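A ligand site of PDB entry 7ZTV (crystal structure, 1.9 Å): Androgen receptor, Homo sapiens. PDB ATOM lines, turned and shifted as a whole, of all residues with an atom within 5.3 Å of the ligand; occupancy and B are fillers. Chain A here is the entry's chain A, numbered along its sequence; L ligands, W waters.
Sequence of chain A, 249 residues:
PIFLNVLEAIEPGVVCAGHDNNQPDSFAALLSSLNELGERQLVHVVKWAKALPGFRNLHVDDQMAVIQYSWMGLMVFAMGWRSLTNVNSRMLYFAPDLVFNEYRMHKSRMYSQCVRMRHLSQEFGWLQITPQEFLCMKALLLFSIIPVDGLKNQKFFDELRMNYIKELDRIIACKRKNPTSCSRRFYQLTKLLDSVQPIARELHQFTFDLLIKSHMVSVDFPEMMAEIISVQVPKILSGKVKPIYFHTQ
O1 of the ligand sits at hydrogen-bond distance from NH2 of Arg 82.
An oxygen (O2) of the ligand lies within hydrogen-bond range of the side-chain hydroxyl of Thr 207, 2.6 Å away.
An oxygen (O2) of the ligand lies within hydrogen-bond range of the side-chain amide oxygen (OD1) of Asn 35.
The guanidinium group of Arg 82 lies close to the side-chain amide nitrogen of Gln 41 (3.1 Å).
SD of Met 75 sits close to OE1 of Gln 41, at 3.6 Å.
The guanidinium group (NH2) of Arg 82 sits at hydrogen-bond distance from the backbone carbonyl oxygen (O) of Phe 94.
O of Leu 31 lies close to ND2 of Asn 35 (3.4 Å).
Merely in contact with the ligand: Leu 34 (3.4 Å), Gln 41 (3.5 Å), Met 79 (3.5 Å), Met 75 (3.6 Å), Phe 94 (3.7 Å), Met 72 (3.8 Å), Leu 37 (3.8 Å), Phe 206 (3.9 Å), Leu 31 (3.9 Å), Met 110 (3.9 Å), Met 225 (3.9 Å) and Leu 210 (3.9 Å).
Hydrophobic or aromatic side chains that line the ligand: Leu 31, Leu 37, Met 72, Met 75, Met 79, Phe 94, Met 110, Phe 206, Leu 210 and Met 225.
Of the 22 residues printed, 15 come within 4 Å of the ligand.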
ATOM      1  N   LEU A  31       0.346 -12.955   9.685  1.00  0.00           N
ATOM      2  CA  LEU A  31       0.745 -14.133   8.924  1.00  0.00           C
ATOM      3  C   LEU A  31      -0.102 -15.346   9.294  1.00  0.00           C
ATOM      4  O   LEU A  31      -0.367 -16.185   8.446  1.00  0.00           O
ATOM      5  CB  LEU A  31       2.251 -14.355   9.065  1.00  0.00           C
ATOM      6  CG  LEU A  31       3.120 -13.751   7.951  1.00  0.00           C
ATOM      7  CD1 LEU A  31       2.810 -14.383   6.610  1.00  0.00           C
ATOM      8  CD2 LEU A  31       2.956 -12.248   7.846  1.00  0.00           C
ATOM      9  N   LEU A  34      -3.151 -14.845   7.147  1.00  0.00           N
ATOM     10  CA  LEU A  34      -2.907 -15.240   5.753  1.00  0.00           C
ATOM     11  C   LEU A  34      -2.881 -16.772   5.639  1.00  0.00           C
ATOM     12  O   LEU A  34      -3.392 -17.330   4.675  1.00  0.00           O
ATOM     13  CB  LEU A  34      -1.587 -14.656   5.261  1.00  0.00           C
ATOM     14  CG  LEU A  34      -1.599 -13.149   4.954  1.00  0.00           C
ATOM     15  CD1 LEU A  34      -0.220 -12.656   4.542  1.00  0.00           C
ATOM     16  CD2 LEU A  34      -2.592 -12.795   3.845  1.00  0.00           C
ATOM     17  N   ASN A  35      -2.261 -17.461   6.604  1.00  0.00           N
ATOM     18  CA  ASN A  35      -2.184 -18.921   6.552  1.00  0.00           C
ATOM     19  C   ASN A  35      -3.589 -19.514   6.671  1.00  0.00           C
ATOM     20  O   ASN A  35      -3.898 -20.473   5.979  1.00  0.00           O
ATOM     21  CB  ASN A  35      -1.279 -19.484   7.642  1.00  0.00           C
ATOM     22  CG  ASN A  35       0.181 -19.251   7.361  1.00  0.00           C
ATOM     23  OD1 ASN A  35       0.589 -19.027   6.219  1.00  0.00           O
ATOM     24  ND2 ASN A  35       0.991 -19.260   8.412  1.00  0.00           N
ATOM     25  N   LEU A  37      -6.375 -17.978   5.783  1.00  0.00           N
ATOM     26  CA  LEU A  37      -6.956 -17.659   4.497  1.00  0.00           C
ATOM     27  C   LEU A  37      -6.525 -18.692   3.459  1.00  0.00           C
ATOM     28  O   LEU A  37      -7.347 -19.186   2.684  1.00  0.00           O
ATOM     29  CB  LEU A  37      -6.493 -16.253   4.061  1.00  0.00           C
ATOM     30  CG  LEU A  37      -6.977 -15.831   2.665  1.00  0.00           C
ATOM     31  CD1 LEU A  37      -8.491 -16.047   2.509  1.00  0.00           C
ATOM     32  CD2 LEU A  37      -6.649 -14.393   2.385  1.00  0.00           C
ATOM     33  N   GLY A  38      -5.223 -18.986   3.413  1.00  0.00           N
ATOM     34  CA  GLY A  38      -4.690 -20.004   2.504  1.00  0.00           C
ATOM     35  C   GLY A  38      -5.414 -21.350   2.667  1.00  0.00           C
ATOM     36  O   GLY A  38      -5.810 -21.964   1.678  1.00  0.00           O
ATOM     37  N   GLN A  41      -8.972 -21.026   1.328  1.00  0.00           N
ATOM     38  CA  GLN A  41      -8.953 -20.887  -0.114  1.00  0.00           C
ATOM     39  C   GLN A  41      -8.591 -22.220  -0.770  1.00  0.00           C
ATOM     40  O   GLN A  41      -9.118 -22.540  -1.823  1.00  0.00           O
ATOM     41  CB  GLN A  41      -8.064 -19.736  -0.562  1.00  0.00           C
ATOM     42  CG  GLN A  41      -8.770 -18.386  -0.438  1.00  0.00           C
ATOM     43  CD  GLN A  41      -8.171 -17.364  -1.367  1.00  0.00           C
ATOM     44  OE1 GLN A  41      -7.353 -17.693  -2.219  1.00  0.00           O
ATOM     45  NE2 GLN A  41      -8.596 -16.118  -1.228  1.00  0.00           N
ATOM     46  N   TRP A  71      -1.211 -24.005  -6.481  1.00  0.00           N
ATOM     47  CA  TRP A  71      -2.170 -23.240  -5.701  1.00  0.00           C
ATOM     48  C   TRP A  71      -1.689 -21.815  -5.464  1.00  0.00           C
ATOM     49  O   TRP A  71      -2.492 -20.892  -5.436  1.00  0.00           O
ATOM     50  CB  TRP A  71      -2.493 -23.927  -4.390  1.00  0.00           C
ATOM     51  CG  TRP A  71      -1.290 -24.101  -3.528  1.00  0.00           C
ATOM     52  CD1 TRP A  71      -0.357 -25.093  -3.613  1.00  0.00           C
ATOM     53  CD2 TRP A  71      -0.844 -23.221  -2.471  1.00  0.00           C
ATOM     54  NE1 TRP A  71       0.620 -24.920  -2.665  1.00  0.00           N
ATOM     55  CE2 TRP A  71       0.338 -23.792  -1.937  1.00  0.00           C
ATOM     56  CE3 TRP A  71      -1.348 -22.065  -1.882  1.00  0.00           C
ATOM     57  CZ2 TRP A  71       1.036 -23.197  -0.878  1.00  0.00           C
ATOM     58  CZ3 TRP A  71      -0.669 -21.478  -0.832  1.00  0.00           C
ATOM     59  CH2 TRP A  71       0.497 -22.053  -0.328  1.00  0.00           C
ATOM     60  N   MET A  72      -0.378 -21.634  -5.240  1.00  0.00           N
ATOM     61  CA  MET A  72       0.079 -20.315  -4.846  1.00  0.00           C
ATOM     62  C   MET A  72      -0.181 -19.324  -5.982  1.00  0.00           C
ATOM     63  O   MET A  72      -0.759 -18.264  -5.766  1.00  0.00           O
ATOM     64  CB  MET A  72       1.572 -20.312  -4.488  1.00  0.00           C
ATOM     65  CG  MET A  72       2.091 -18.920  -4.168  1.00  0.00           C
ATOM     66  SD  MET A  72       1.689 -18.469  -2.468  1.00  0.00           S
ATOM     67  CE  MET A  72       2.816 -19.559  -1.575  1.00  0.00           C
ATOM     68  N   MET A  75      -3.963 -18.568  -6.450  1.00  0.00           N
ATOM     69  CA  MET A  75      -4.494 -17.690  -5.419  1.00  0.00           C
ATOM     70  C   MET A  75      -3.993 -16.260  -5.578  1.00  0.00           C
ATOM     71  O   MET A  75      -4.740 -15.314  -5.385  1.00  0.00           O
ATOM     72  CB  MET A  75      -4.163 -18.230  -4.022  1.00  0.00           C
ATOM     73  CG  MET A  75      -4.902 -19.524  -3.696  1.00  0.00           C
ATOM     74  SD  MET A  75      -4.592 -19.964  -1.963  1.00  0.00           S
ATOM     75  CE  MET A  75      -5.123 -21.685  -1.939  1.00  0.00           C
ATOM     76  N   VAL A  76      -2.729 -16.104  -5.971  1.00  0.00           N
ATOM     77  CA  VAL A  76      -2.176 -14.778  -6.200  1.00  0.00           C
ATOM     78  C   VAL A  76      -2.863 -14.106  -7.390  1.00  0.00           C
ATOM     79  O   VAL A  76      -3.195 -12.917  -7.329  1.00  0.00           O
ATOM     80  CB  VAL A  76      -0.665 -14.853  -6.428  1.00  0.00           C
ATOM     81  CG1 VAL A  76      -0.145 -13.523  -6.973  1.00  0.00           C
ATOM     82  CG2 VAL A  76       0.036 -15.144  -5.127  1.00  0.00           C
ATOM     83  N   MET A  79      -6.294 -13.046  -6.454  1.00  0.00           N
ATOM     84  CA  MET A  79      -6.242 -11.982  -5.470  1.00  0.00           C
ATOM     85  C   MET A  79      -6.003 -10.637  -6.162  1.00  0.00           C
ATOM     86  O   MET A  79      -6.682  -9.659  -5.884  1.00  0.00           O
ATOM     87  CB  MET A  79      -5.133 -12.245  -4.451  1.00  0.00           C
ATOM     88  CG  MET A  79      -5.121 -11.218  -3.337  1.00  0.00           C
ATOM     89  SD  MET A  79      -4.049  -9.819  -3.721  1.00  0.00           S
ATOM     90  CE  MET A  79      -2.452 -10.613  -3.517  1.00  0.00           C
ATOM     91  N   ARG A  82      -9.377  -9.594  -7.637  1.00  0.00           N
ATOM     92  CA  ARG A  82     -10.240  -9.004  -6.621  1.00  0.00           C
ATOM     93  C   ARG A  82      -9.730  -7.606  -6.311  1.00  0.00           C
ATOM     94  O   ARG A  82     -10.510  -6.666  -6.166  1.00  0.00           O
ATOM     95  CB  ARG A  82     -10.138  -9.678  -5.247  1.00  0.00           C
ATOM     96  CG  ARG A  82     -10.574 -11.117  -5.185  1.00  0.00           C
ATOM     97  CD  ARG A  82     -10.786 -11.480  -3.739  1.00  0.00           C
ATOM     98  NE  ARG A  82      -9.596 -11.945  -3.060  1.00  0.00           N
ATOM     99  CZ  ARG A  82      -8.982 -13.089  -3.309  1.00  0.00           C
ATOM    100  NH1 ARG A  82      -9.423 -13.905  -4.267  1.00  0.00           N
ATOM    101  NH2 ARG A  82      -7.917 -13.426  -2.603  1.00  0.00           N
ATOM    102  N   PHE A  94      -6.828  -9.239   0.155  1.00  0.00           N
ATOM    103  CA  PHE A  94      -6.685 -10.674   0.334  1.00  0.00           C
ATOM    104  C   PHE A  94      -8.064 -11.283   0.546  1.00  0.00           C
ATOM    105  O   PHE A  94      -8.404 -12.281  -0.080  1.00  0.00           O
ATOM    106  CB  PHE A  94      -5.659 -10.989   1.428  1.00  0.00           C
ATOM    107  CG  PHE A  94      -4.216 -10.691   1.055  1.00  0.00           C
ATOM    108  CD1 PHE A  94      -3.529 -11.470   0.134  1.00  0.00           C
ATOM    109  CD2 PHE A  94      -3.537  -9.641   1.645  1.00  0.00           C
ATOM    110  CE1 PHE A  94      -2.205 -11.212  -0.186  1.00  0.00           C
ATOM    111  CE2 PHE A  94      -2.210  -9.357   1.307  1.00  0.00           C
ATOM    112  CZ  PHE A  94      -1.538 -10.160   0.417  1.00  0.00           C
ATOM    113  N   MET A 110       6.609  -8.517   4.167  1.00  0.00           N
ATOM    114  CA  MET A 110       6.512  -9.033   2.819  1.00  0.00           C
ATOM    115  C   MET A 110       6.431  -7.873   1.838  1.00  0.00           C
ATOM    116  O   MET A 110       5.771  -7.967   0.797  1.00  0.00           O
ATOM    117  CB  MET A 110       5.250  -9.883   2.666  1.00  0.00           C
ATOM    118  CG  MET A 110       5.469 -11.318   3.008  1.00  0.00           C
ATOM    119  SD  MET A 110       4.009 -12.264   2.564  1.00  0.00           S
ATOM    120  CE  MET A 110       2.849 -11.692   3.798  1.00  0.00           C
ATOM    121  N   MET A 117       2.964  -8.204  -6.229  1.00  0.00           N
ATOM    122  CA  MET A 117       1.558  -8.585  -6.366  1.00  0.00           C
ATOM    123  C   MET A 117       0.713  -7.383  -6.791  1.00  0.00           C
ATOM    124  O   MET A 117      -0.204  -7.509  -7.607  1.00  0.00           O
ATOM    125  CB  MET A 117       1.015  -9.206  -5.076  1.00  0.00           C
ATOM    126  CG  MET A 117       1.810 -10.421  -4.657  1.00  0.00           C
ATOM    127  SD  MET A 117       0.938 -11.470  -3.463  1.00  0.00           S
ATOM    128  CE  MET A 117       1.610 -10.894  -1.905  1.00  0.00           C
ATOM    129  N   LEU A 203       7.039 -16.233  -3.038  1.00  0.00           N
ATOM    130  CA  LEU A 203       6.177 -16.512  -1.906  1.00  0.00           C
ATOM    131  C   LEU A 203       6.436 -17.918  -1.360  1.00  0.00           C
ATOM    132  O   LEU A 203       6.374 -18.142  -0.164  1.00  0.00           O
ATOM    133  CB  LEU A 203       4.710 -16.263  -2.298  1.00  0.00           C
ATOM    134  CG  LEU A 203       4.372 -14.788  -2.527  1.00  0.00           C
ATOM    135  CD1 LEU A 203       3.070 -14.637  -3.270  1.00  0.00           C
ATOM    136  CD2 LEU A 203       4.379 -13.972  -1.245  1.00  0.00           C
ATOM    137  N   PHE A 206       9.353 -17.559   0.733  1.00  0.00           N
ATOM    138  CA  PHE A 206       8.962 -16.891   1.969  1.00  0.00           C
ATOM    139  C   PHE A 206       8.209 -17.829   2.912  1.00  0.00           C
ATOM    140  O   PHE A 206       8.510 -17.882   4.116  1.00  0.00           O
ATOM    141  CB  PHE A 206       8.156 -15.643   1.623  1.00  0.00           C
ATOM    142  CG  PHE A 206       7.894 -14.763   2.810  1.00  0.00           C
ATOM    143  CD1 PHE A 206       6.805 -15.009   3.642  1.00  0.00           C
ATOM    144  CD2 PHE A 206       8.766 -13.743   3.131  1.00  0.00           C
ATOM    145  CE1 PHE A 206       6.575 -14.206   4.752  1.00  0.00           C
ATOM    146  CE2 PHE A 206       8.545 -12.945   4.251  1.00  0.00           C
ATOM    147  CZ  PHE A 206       7.440 -13.188   5.058  1.00  0.00           C
ATOM    148  N   THR A 207       7.194 -18.552   2.402  1.00  0.00           N
ATOM    149  CA  THR A 207       6.331 -19.354   3.279  1.00  0.00           C
ATOM    150  C   THR A 207       7.118 -20.553   3.810  1.00  0.00           C
ATOM    151  O   THR A 207       6.921 -20.996   4.960  1.00  0.00           O
ATOM    152  CB  THR A 207       5.030 -19.789   2.588  1.00  0.00           C
ATOM    153  OG1 THR A 207       4.127 -20.229   3.592  1.00  0.00           O
ATOM    154  CG2 THR A 207       5.185 -20.954   1.636  1.00  0.00           C
ATOM    155  N   LEU A 210       9.318 -19.358   6.622  1.00  0.00           N
ATOM    156  CA  LEU A 210       8.451 -19.033   7.728  1.00  0.00           C
ATOM    157  C   LEU A 210       7.985 -20.297   8.446  1.00  0.00           C
ATOM    158  O   LEU A 210       7.881 -20.262   9.654  1.00  0.00           O
ATOM    159  CB  LEU A 210       7.273 -18.230   7.167  1.00  0.00           C
ATOM    160  CG  LEU A 210       6.211 -17.782   8.159  1.00  0.00           C
ATOM    161  CD1 LEU A 210       6.774 -16.880   9.239  1.00  0.00           C
ATOM    162  CD2 LEU A 210       5.091 -17.077   7.420  1.00  0.00           C
ATOM    163  N   PHE A 221       0.284 -22.357  11.421  1.00  0.00           N
ATOM    164  CA  PHE A 221       0.089 -22.937  10.111  1.00  0.00           C
ATOM    165  C   PHE A 221      -0.964 -24.036  10.244  1.00  0.00           C
ATOM    166  O   PHE A 221      -0.711 -25.048  10.897  1.00  0.00           O
ATOM    167  CB  PHE A 221       1.418 -23.525   9.621  1.00  0.00           C
ATOM    168  CG  PHE A 221       2.299 -22.574   8.833  1.00  0.00           C
ATOM    169  CD1 PHE A 221       3.233 -21.795   9.475  1.00  0.00           C
ATOM    170  CD2 PHE A 221       2.187 -22.494   7.452  1.00  0.00           C
ATOM    171  CE1 PHE A 221       4.044 -20.933   8.747  1.00  0.00           C
ATOM    172  CE2 PHE A 221       3.007 -21.647   6.728  1.00  0.00           C
ATOM    173  CZ  PHE A 221       3.941 -20.882   7.371  1.00  0.00           C
ATOM    174  N   MET A 225      -1.967 -26.680   5.091  1.00  0.00           N
ATOM    175  CA  MET A 225      -0.884 -25.760   4.765  1.00  0.00           C
ATOM    176  C   MET A 225       0.465 -26.328   5.201  1.00  0.00           C
ATOM    177  O   MET A 225       1.413 -26.341   4.430  1.00  0.00           O
ATOM    178  CB  MET A 225      -1.106 -24.392   5.430  1.00  0.00           C
ATOM    179  CG  MET A 225      -2.282 -23.613   4.852  1.00  0.00           C
ATOM    180  SD  MET A 225      -2.024 -23.201   3.109  1.00  0.00           S
ATOM    181  CE  MET A 225      -1.085 -21.690   3.330  1.00  0.00           C
ATOM    182  N   ILE A 229       3.314 -27.303   2.450  1.00  0.00           N
ATOM    183  CA  ILE A 229       4.486 -26.473   2.397  1.00  0.00           C
ATOM    184  C   ILE A 229       5.745 -27.272   2.760  1.00  0.00           C
ATOM    185  O   ILE A 229       6.826 -26.920   2.309  1.00  0.00           O
ATOM    186  CB  ILE A 229       4.299 -25.211   3.228  1.00  0.00           C
ATOM    187  CG1 ILE A 229       3.231 -24.343   2.544  1.00  0.00           C
ATOM    188  CG2 ILE A 229       5.625 -24.477   3.430  1.00  0.00           C
ATOM    189  CD1 ILE A 229       2.721 -23.224   3.369  1.00  0.00           C
HETATM  190  C1  LIG L   1      -3.729 -16.404   0.682  1.00  0.00           C
HETATM  191  C2  LIG L   1      -4.796 -16.209  -0.408  1.00  0.00           C
HETATM  192  C3  LIG L   1      -4.541 -15.011  -1.271  1.00  0.00           C
HETATM  193  O1  LIG L   1      -5.403 -14.191  -1.518  1.00  0.00           O
HETATM  194  C4  LIG L   1      -3.137 -14.862  -1.787  1.00  0.00           C
HETATM  195  C5  LIG L   1      -2.107 -15.056  -0.652  1.00  0.00           C
HETATM  196  C6  LIG L   1      -0.672 -14.777  -1.103  1.00  0.00           C
HETATM  197  C7  LIG L   1       0.278 -14.803   0.095  1.00  0.00           C
HETATM  198  C8  LIG L   1       0.205 -16.131   0.824  1.00  0.00           C
HETATM  199  C9  LIG L   1      -1.230 -16.469   1.270  1.00  0.00           C
HETATM  200  C10 LIG L   1      -2.287 -16.390   0.120  1.00  0.00           C
HETATM  201  C11 LIG L   1      -1.277 -17.807   2.034  1.00  0.00           C
HETATM  202  C12 LIG L   1      -0.272 -17.876   3.196  1.00  0.00           C
HETATM  203  C13 LIG L   1       1.151 -17.522   2.761  1.00  0.00           C
HETATM  204  C14 LIG L   1       1.100 -16.167   2.044  1.00  0.00           C
HETATM  205  C15 LIG L   1       2.581 -15.802   1.891  1.00  0.00           C
HETATM  206  C16 LIG L   1       3.171 -16.261   3.251  1.00  0.00           C
HETATM  207  C17 LIG L   1       2.099 -17.148   3.906  1.00  0.00           C
HETATM  208  O2  LIG L   1       2.705 -18.246   4.561  1.00  0.00           O
HETATM  209  C18 LIG L   1       1.791 -18.657   1.944  1.00  0.00           C
HETATM  210  C19 LIG L   1      -2.132 -17.591  -0.834  1.00  0.00           C
HETATM  211  O   HOH W   1      -7.117 -15.793  -4.007  1.00  0.00           O
